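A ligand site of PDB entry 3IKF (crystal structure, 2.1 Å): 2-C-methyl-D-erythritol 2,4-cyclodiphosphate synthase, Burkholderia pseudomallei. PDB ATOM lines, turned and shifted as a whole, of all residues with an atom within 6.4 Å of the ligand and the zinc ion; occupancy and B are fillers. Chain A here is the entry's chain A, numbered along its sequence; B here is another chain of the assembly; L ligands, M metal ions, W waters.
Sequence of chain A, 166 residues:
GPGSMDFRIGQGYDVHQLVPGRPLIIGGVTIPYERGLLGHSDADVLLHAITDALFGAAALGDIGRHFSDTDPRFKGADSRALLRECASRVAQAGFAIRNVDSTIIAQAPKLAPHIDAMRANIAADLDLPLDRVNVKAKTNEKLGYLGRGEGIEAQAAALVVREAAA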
ATOM      1  N   ASP A  14      -9.828  22.893 -19.186  1.00  0.00           N
ATOM      2  CA  ASP A  14      -9.708  21.807 -20.122  1.00  0.00           C
ATOM      3  C   ASP A  14     -10.959  20.905 -20.107  1.00  0.00           C
ATOM      4  O   ASP A  14     -11.640  20.801 -19.092  1.00  0.00           O
ATOM      5  CB  ASP A  14      -8.454  20.983 -19.808  1.00  0.00           C
ATOM      6  CG  ASP A  14      -7.963  20.181 -21.011  1.00  0.00           C
ATOM      7  OD1 ASP A  14      -8.277  20.512 -22.164  1.00  0.00           O
ATOM      8  OD2 ASP A  14      -7.272  19.191 -20.776  1.00  0.00           O
ATOM      9  N   VAL A  15     -11.269  20.268 -21.240  1.00  0.00           N
ATOM     10  CA  VAL A  15     -12.318  19.237 -21.268  1.00  0.00           C
ATOM     11  C   VAL A  15     -11.854  18.169 -22.241  1.00  0.00           C
ATOM     12  O   VAL A  15     -11.224  18.504 -23.246  1.00  0.00           O
ATOM     13  CB  VAL A  15     -13.726  19.826 -21.678  1.00  0.00           C
ATOM     14  CG1 VAL A  15     -13.708  20.359 -23.123  1.00  0.00           C
ATOM     15  CG2 VAL A  15     -14.847  18.784 -21.500  1.00  0.00           C
ATOM     16  N   HIS A  16     -12.098  16.905 -21.912  1.00  0.00           N
ATOM     17  CA  HIS A  16     -11.891  15.786 -22.826  1.00  0.00           C
ATOM     18  C   HIS A  16     -13.136  14.929 -22.835  1.00  0.00           C
ATOM     19  O   HIS A  16     -13.868  14.866 -21.838  1.00  0.00           O
ATOM     20  CB  HIS A  16     -10.714  14.897 -22.396  1.00  0.00           C
ATOM     21  CG  HIS A  16      -9.372  15.530 -22.616  1.00  0.00           C
ATOM     22  ND1 HIS A  16      -8.606  15.266 -23.732  1.00  0.00           N
ATOM     23  CD2 HIS A  16      -8.684  16.439 -21.881  1.00  0.00           C
ATOM     24  CE1 HIS A  16      -7.491  15.984 -23.673  1.00  0.00           C
ATOM     25  NE2 HIS A  16      -7.520  16.715 -22.565  1.00  0.00           N
ATOM     26  N   LEU A  38     -10.330  10.858 -23.700  1.00  0.00           N
ATOM     27  CA  LEU A  38      -9.774  10.751 -25.047  1.00  0.00           C
ATOM     28  C   LEU A  38      -8.917  11.944 -25.358  1.00  0.00           C
ATOM     29  O   LEU A  38      -9.383  13.086 -25.293  1.00  0.00           O
ATOM     30  CB  LEU A  38     -10.896  10.641 -26.081  1.00  0.00           C
ATOM     31  CG  LEU A  38     -10.427  10.729 -27.547  1.00  0.00           C
ATOM     32  CD1 LEU A  38      -9.711   9.425 -27.951  1.00  0.00           C
ATOM     33  CD2 LEU A  38     -11.616  11.033 -28.499  1.00  0.00           C
ATOM     34  N   HIS A  40      -4.728  13.012 -27.388  1.00  0.00           N
ATOM     35  CA  HIS A  40      -3.409  12.673 -27.950  1.00  0.00           C
ATOM     36  C   HIS A  40      -2.404  12.142 -26.896  1.00  0.00           C
ATOM     37  O   HIS A  40      -1.780  11.085 -27.104  1.00  0.00           O
ATOM     38  CB  HIS A  40      -2.854  13.918 -28.637  1.00  0.00           C
ATOM     39  CG  HIS A  40      -1.569  13.713 -29.367  1.00  0.00           C
ATOM     40  ND1 HIS A  40      -1.475  12.939 -30.502  1.00  0.00           N
ATOM     41  CD2 HIS A  40      -0.340  14.239 -29.164  1.00  0.00           C
ATOM     42  CE1 HIS A  40      -0.232  12.962 -30.951  1.00  0.00           C
ATOM     43  NE2 HIS A  40       0.487  13.745 -30.162  1.00  0.00           N
ATOM     44  N   SER A  41      -2.278  12.872 -25.783  1.00  0.00           N
ATOM     45  CA  SER A  41      -1.480  12.437 -24.631  1.00  0.00           C
ATOM     46  C   SER A  41      -2.359  11.524 -23.778  1.00  0.00           C
ATOM     47  O   SER A  41      -3.392  11.045 -24.276  1.00  0.00           O
ATOM     48  CB  SER A  41      -1.007  13.649 -23.803  1.00  0.00           C
ATOM     49  OG  SER A  41      -2.085  14.334 -23.178  1.00  0.00           O
ATOM     50  N   ALA A  43      -4.357  12.388 -21.801  1.00  0.00           N
ATOM     51  CA  ALA A  43      -5.650  13.112 -21.735  1.00  0.00           C
ATOM     52  C   ALA A  43      -6.072  13.543 -20.309  1.00  0.00           C
ATOM     53  O   ALA A  43      -7.265  13.764 -20.018  1.00  0.00           O
ATOM     54  CB  ALA A  43      -6.792  12.323 -22.457  1.00  0.00           C
ATOM     55  N   ASP A  44      -5.082  13.716 -19.447  1.00  0.00           N
ATOM     56  CA  ASP A  44      -5.323  14.065 -18.050  1.00  0.00           C
ATOM     57  C   ASP A  44      -5.820  15.499 -17.949  1.00  0.00           C
ATOM     58  O   ASP A  44      -5.026  16.451 -17.923  1.00  0.00           O
ATOM     59  CB  ASP A  44      -4.019  13.851 -17.251  1.00  0.00           C
ATOM     60  CG  ASP A  44      -4.243  13.898 -15.739  1.00  0.00           C
ATOM     61  OD1 ASP A  44      -5.092  14.683 -15.279  1.00  0.00           O
ATOM     62  OD2 ASP A  44      -3.536  13.165 -15.019  1.00  0.00           O
ATOM     63  N   VAL A  45      -7.142  15.647 -17.916  1.00  0.00           N
ATOM     64  CA  VAL A  45      -7.788  16.967 -18.019  1.00  0.00           C
ATOM     65  C   VAL A  45      -7.398  17.924 -16.860  1.00  0.00           C
ATOM     66  O   VAL A  45      -7.257  19.132 -17.055  1.00  0.00           O
ATOM     67  CB  VAL A  45      -9.347  16.798 -18.168  1.00  0.00           C
ATOM     68  CG1 VAL A  45      -9.974  16.111 -16.923  1.00  0.00           C
ATOM     69  CG2 VAL A  45     -10.039  18.104 -18.454  1.00  0.00           C
ATOM     70  N   HIS A  48      -3.714  19.177 -17.303  1.00  0.00           N
ATOM     71  CA  HIS A  48      -3.631  20.110 -18.410  1.00  0.00           C
ATOM     72  C   HIS A  48      -4.133  21.497 -18.014  1.00  0.00           C
ATOM     73  O   HIS A  48      -3.551  22.515 -18.379  1.00  0.00           O
ATOM     74  CB  HIS A  48      -4.456  19.589 -19.631  1.00  0.00           C
ATOM     75  CG  HIS A  48      -3.894  18.336 -20.241  1.00  0.00           C
ATOM     76  ND1 HIS A  48      -4.529  17.645 -21.250  1.00  0.00           N
ATOM     77  CD2 HIS A  48      -2.750  17.651 -19.964  1.00  0.00           C
ATOM     78  CE1 HIS A  48      -3.804  16.581 -21.571  1.00  0.00           C
ATOM     79  NE2 HIS A  48      -2.728  16.556 -20.790  1.00  0.00           N
ATOM     80  N   ALA A  49      -5.253  21.502 -17.282  1.00  0.00           N
ATOM     81  CA  ALA A  49      -5.832  22.731 -16.780  1.00  0.00           C
ATOM     82  C   ALA A  49      -4.842  23.442 -15.814  1.00  0.00           C
ATOM     83  O   ALA A  49      -4.657  24.677 -15.889  1.00  0.00           O
ATOM     84  CB  ALA A  49      -7.196  22.421 -16.078  1.00  0.00           C
ATOM     85  N   ILE A  63      -0.546  25.366 -23.020  1.00  0.00           N
ATOM     86  CA  ILE A  63      -0.098  23.983 -23.081  1.00  0.00           C
ATOM     87  C   ILE A  63      -0.222  23.452 -24.523  1.00  0.00           C
ATOM     88  O   ILE A  63       0.580  22.624 -24.954  1.00  0.00           O
ATOM     89  CB  ILE A  63      -0.947  23.082 -22.144  1.00  0.00           C
ATOM     90  CG1 ILE A  63      -0.285  21.719 -21.962  1.00  0.00           C
ATOM     91  CG2 ILE A  63      -2.433  23.003 -22.641  1.00  0.00           C
ATOM     92  CD1 ILE A  63      -1.070  20.765 -21.030  1.00  0.00           C
ATOM     93  N   GLY A  64      -1.230  23.933 -25.253  1.00  0.00           N
ATOM     94  CA  GLY A  64      -1.437  23.522 -26.651  1.00  0.00           C
ATOM     95  C   GLY A  64      -0.246  23.874 -27.515  1.00  0.00           C
ATOM     96  O   GLY A  64       0.034  23.193 -28.503  1.00  0.00           O
ATOM     97  N   ARG A  65       0.490  24.906 -27.101  1.00  0.00           N
ATOM     98  CA  ARG A  65       1.689  25.384 -27.780  1.00  0.00           C
ATOM     99  C   ARG A  65       3.008  24.746 -27.302  1.00  0.00           C
ATOM    100  O   ARG A  65       3.868  24.390 -28.124  1.00  0.00           O
ATOM    101  CB  ARG A  65       1.772  26.889 -27.578  1.00  0.00           C
ATOM    102  CG  ARG A  65       3.129  27.493 -27.824  1.00  0.00           C
ATOM    103  CD  ARG A  65       3.201  28.808 -27.091  1.00  0.00           C
ATOM    104  NE  ARG A  65       4.572  29.234 -26.828  1.00  0.00           N
ATOM    105  CZ  ARG A  65       4.920  30.490 -26.554  1.00  0.00           C
ATOM    106  NH1 ARG A  65       6.195  30.805 -26.308  1.00  0.00           N
ATOM    107  NH2 ARG A  65       3.995  31.439 -26.546  1.00  0.00           N
ATOM    108  N   PHE A  67       3.223  21.918 -25.696  1.00  0.00           N
ATOM    109  CA  PHE A  67       3.087  20.463 -25.816  1.00  0.00           C
ATOM    110  C   PHE A  67       1.947  20.092 -26.791  1.00  0.00           C
ATOM    111  O   PHE A  67       0.888  19.539 -26.408  1.00  0.00           O
ATOM    112  CB  PHE A  67       2.850  19.831 -24.429  1.00  0.00           C
ATOM    113  CG  PHE A  67       3.826  20.292 -23.346  1.00  0.00           C
ATOM    114  CD1 PHE A  67       5.205  20.197 -23.516  1.00  0.00           C
ATOM    115  CD2 PHE A  67       3.344  20.786 -22.129  1.00  0.00           C
ATOM    116  CE1 PHE A  67       6.091  20.624 -22.484  1.00  0.00           C
ATOM    117  CE2 PHE A  67       4.230  21.214 -21.097  1.00  0.00           C
ATOM    118  CZ  PHE A  67       5.584  21.115 -21.278  1.00  0.00           C
ATOM    119  N   SER A  68       2.176  20.394 -28.071  1.00  0.00           N
ATOM    120  CA  SER A  68       1.123  20.315 -29.109  1.00  0.00           C
ATOM    121  C   SER A  68       0.450  18.945 -29.296  1.00  0.00           C
ATOM    122  O   SER A  68       1.130  17.903 -29.273  1.00  0.00           O
ATOM    123  CB  SER A  68       1.681  20.852 -30.435  1.00  0.00           C
ATOM    124  OG  SER A  68       0.789  20.602 -31.517  1.00  0.00           O
ATOM    125  N   ASP A  69      -0.868  18.933 -29.482  1.00  0.00           N
ATOM    126  CA  ASP A  69      -1.582  17.686 -29.715  1.00  0.00           C
ATOM    127  C   ASP A  69      -1.409  17.198 -31.149  1.00  0.00           C
ATOM    128  O   ASP A  69      -1.914  16.143 -31.512  1.00  0.00           O
ATOM    129  CB  ASP A  69      -3.065  17.736 -29.310  1.00  0.00           C
ATOM    130  CG  ASP A  69      -3.854  18.845 -29.994  1.00  0.00           C
ATOM    131  OD1 ASP A  69      -3.376  19.474 -30.971  1.00  0.00           O
ATOM    132  OD2 ASP A  69      -4.983  19.097 -29.527  1.00  0.00           O
ATOM    133  N   SER A  79       1.143  13.180 -18.588  1.00  0.00           N
ATOM    134  CA  SER A  79       0.862  14.581 -18.299  1.00  0.00           C
ATOM    135  C   SER A  79       1.496  15.092 -17.002  1.00  0.00           C
ATOM    136  O   SER A  79       1.575  16.310 -16.781  1.00  0.00           O
ATOM    137  CB  SER A  79      -0.649  14.832 -18.277  1.00  0.00           C
ATOM    138  OG  SER A  79      -1.196  14.696 -19.592  1.00  0.00           O
ATOM    139  N   LEU A  82       4.672  16.298 -18.347  1.00  0.00           N
ATOM    140  CA  LEU A  82       4.360  17.582 -18.956  1.00  0.00           C
ATOM    141  C   LEU A  82       4.229  18.697 -17.900  1.00  0.00           C
ATOM    142  O   LEU A  82       4.784  19.777 -18.055  1.00  0.00           O
ATOM    143  CB  LEU A  82       3.099  17.471 -19.825  1.00  0.00           C
ATOM    144  CG  LEU A  82       3.115  16.537 -21.069  1.00  0.00           C
ATOM    145  CD1 LEU A  82       1.859  16.781 -21.927  1.00  0.00           C
ATOM    146  CD2 LEU A  82       4.367  16.720 -21.916  1.00  0.00           C
ATOM    147  N   LYS B 138      -8.087  27.271 -26.652  1.00  0.00           N
ATOM    148  CA  LYS B 138      -8.602  25.899 -26.470  1.00  0.00           C
ATOM    149  C   LYS B 138      -9.713  25.604 -27.476  1.00  0.00           C
ATOM    150  O   LYS B 138     -10.370  26.516 -27.968  1.00  0.00           O
ATOM    151  CB  LYS B 138      -9.195  25.732 -25.071  1.00  0.00           C
ATOM    152  CG  LYS B 138      -8.239  25.962 -23.884  1.00  0.00           C
ATOM    153  CD  LYS B 138      -7.061  24.974 -23.866  1.00  0.00           C
ATOM    154  CE  LYS B 138      -7.418  23.573 -23.375  1.00  0.00           C
ATOM    155  NZ  LYS B 138      -8.275  22.734 -24.256  1.00  0.00           N
ATOM    156  N   THR B 139      -9.938  24.331 -27.759  1.00  0.00           N
ATOM    157  CA  THR B 139     -11.143  23.892 -28.406  1.00  0.00           C
ATOM    158  C   THR B 139     -11.998  23.227 -27.334  1.00  0.00           C
ATOM    159  O   THR B 139     -11.523  22.994 -26.203  1.00  0.00           O
ATOM    160  CB  THR B 139     -10.895  22.879 -29.570  1.00  0.00           C
ATOM    161  OG1 THR B 139     -10.710  21.563 -29.036  1.00  0.00           O
ATOM    162  CG2 THR B 139      -9.676  23.264 -30.420  1.00  0.00           C
ATOM    163  N   ASN B 140     -13.239  22.893 -27.665  1.00  0.00           N
ATOM    164  CA  ASN B 140     -14.055  22.200 -26.686  1.00  0.00           C
ATOM    165  C   ASN B 140     -14.138  20.703 -26.910  1.00  0.00           C
ATOM    166  O   ASN B 140     -15.023  20.028 -26.344  1.00  0.00           O
ATOM    167  CB  ASN B 140     -15.430  22.831 -26.522  1.00  0.00           C
ATOM    168  CG  ASN B 140     -15.873  22.835 -25.084  1.00  0.00           C
ATOM    169  OD1 ASN B 140     -15.148  23.306 -24.209  1.00  0.00           O
ATOM    170  ND2 ASN B 140     -17.066  22.271 -24.816  1.00  0.00           N
ATOM    171  N   GLU B 141     -13.211  20.182 -27.692  1.00  0.00           N
ATOM    172  CA  GLU B 141     -13.164  18.756 -27.993  1.00  0.00           C
ATOM    173  C   GLU B 141     -14.519  18.237 -28.518  1.00  0.00           C
ATOM    174  O   GLU B 141     -14.936  17.116 -28.211  1.00  0.00           O
ATOM    175  CB  GLU B 141     -12.654  17.950 -26.780  1.00  0.00           C
ATOM    176  CG  GLU B 141     -11.184  18.166 -26.488  1.00  0.00           C
ATOM    177  CD  GLU B 141     -10.288  17.561 -27.570  1.00  0.00           C
ATOM    178  OE1 GLU B 141     -10.359  16.330 -27.772  1.00  0.00           O
ATOM    179  OE2 GLU B 141      -9.519  18.301 -28.209  1.00  0.00           O
HETATM  180  C1  LIG L   1      -6.447  19.229 -24.928  1.00  0.00           C
HETATM  181  N1  LIG L   1      -5.686  19.061 -23.785  1.00  0.00           N
HETATM  182  C2  LIG L   1      -4.414  19.235 -24.270  1.00  0.00           C
HETATM  183  N2  LIG L   1      -4.367  19.490 -25.585  1.00  0.00           N
HETATM  184  C3  LIG L   1      -5.666  19.504 -26.071  1.00  0.00           C
HETATM  185  C4  LIG L   1      -3.105  19.676 -26.168  1.00  0.00           C
HETATM  186  C5  LIG L   1      -2.103  19.555 -25.168  1.00  0.00           C
HETATM  187  S1  LIG L   1      -2.866  19.199 -23.621  1.00  0.00           S
HETATM  188  C6  LIG L   1      -7.947  19.141 -24.937  1.00  0.00           C
HETATM  189  O1  LIG L   1      -8.405  20.345 -25.547  1.00  0.00           O
HETATM  190 ZN    ZN M   1      -6.254  18.246 -22.160  1.00  0.00          ZN
HETATM  191  O   HOH W   1      -0.610  16.956 -26.582  1.00  0.00           O
HETATM  192  O   HOH W   2      -2.285  21.494 -29.011  1.00  0.00           O
HETATM  193  O   HOH W   3      -7.694  22.428 -26.966  1.00  0.00           O
HETATM  194  O   HOH W   4     -10.549  21.082 -24.334  1.00  0.00           O
HETATM  195  O   HOH W   5      -4.606  22.852 -25.096  1.00  0.00           O
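An oxygen (O1) of the ligand lies within hydrogen-bond range of the side-chain amino group (NZ) of Lys 138 of chain B (2.7 Å).
The backbone carbonyl oxygen (O) of Asp 69 lies close to a ring nitrogen (ND1) of His 40 (3.4 Å).
A ring nitrogen (NE2) of His 48 sits at hydrogen-bond distance from the side-chain hydroxyl (OG) of Ser 79 (2.7 Å).
The backbone carbonyl oxygen (O) of Leu 38 sits at hydrogen-bond distance from a ring nitrogen (ND1) of His 16, 2.8 Å away.
OD1 of Asp 14 is in salt-bridge range of NZ of Lys 138 of chain B.
The side-chain hydroxyl (OG) of Ser 41 lies close to a ring nitrogen (NE2) of His 48 (3.3 Å).
The backbone NH of Glu 141 of chain B sits at hydrogen-bond distance from the side-chain hydroxyl of Thr 139 of chain B (3.2 Å).
Residues that only touch the ligand: Phe 67, Ile 63, Glu 141 of chain B, Asp 69 and Val 15.
Nine residues have an atom within 4 Å of the ligand: Asp 14, Val 15, His 16, His 48, Ile 63, Phe 67, Asp 69, Lys 138 of chain B and Glu 141 of chain B.
Within 4 Å of the zinc ion: Asp 14, His 16 and His 48.
The zinc ion is bound by N1 of the ligand (1.9 Å), OD2 of Asp 14 (2.0 Å), NE2 of His 16 (2.0 Å) and ND1 of His 48 (2.0 Å).
Water W3 lies within hydrogen-bond range of O1 of the ligand, NZ of Lys 138 of chain B and N of Thr 139 of chain B.
Water W2 lies within hydrogen-bond range of O of Gly 64 (2.9 Å) and N of Asp 69 (3.0 Å).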
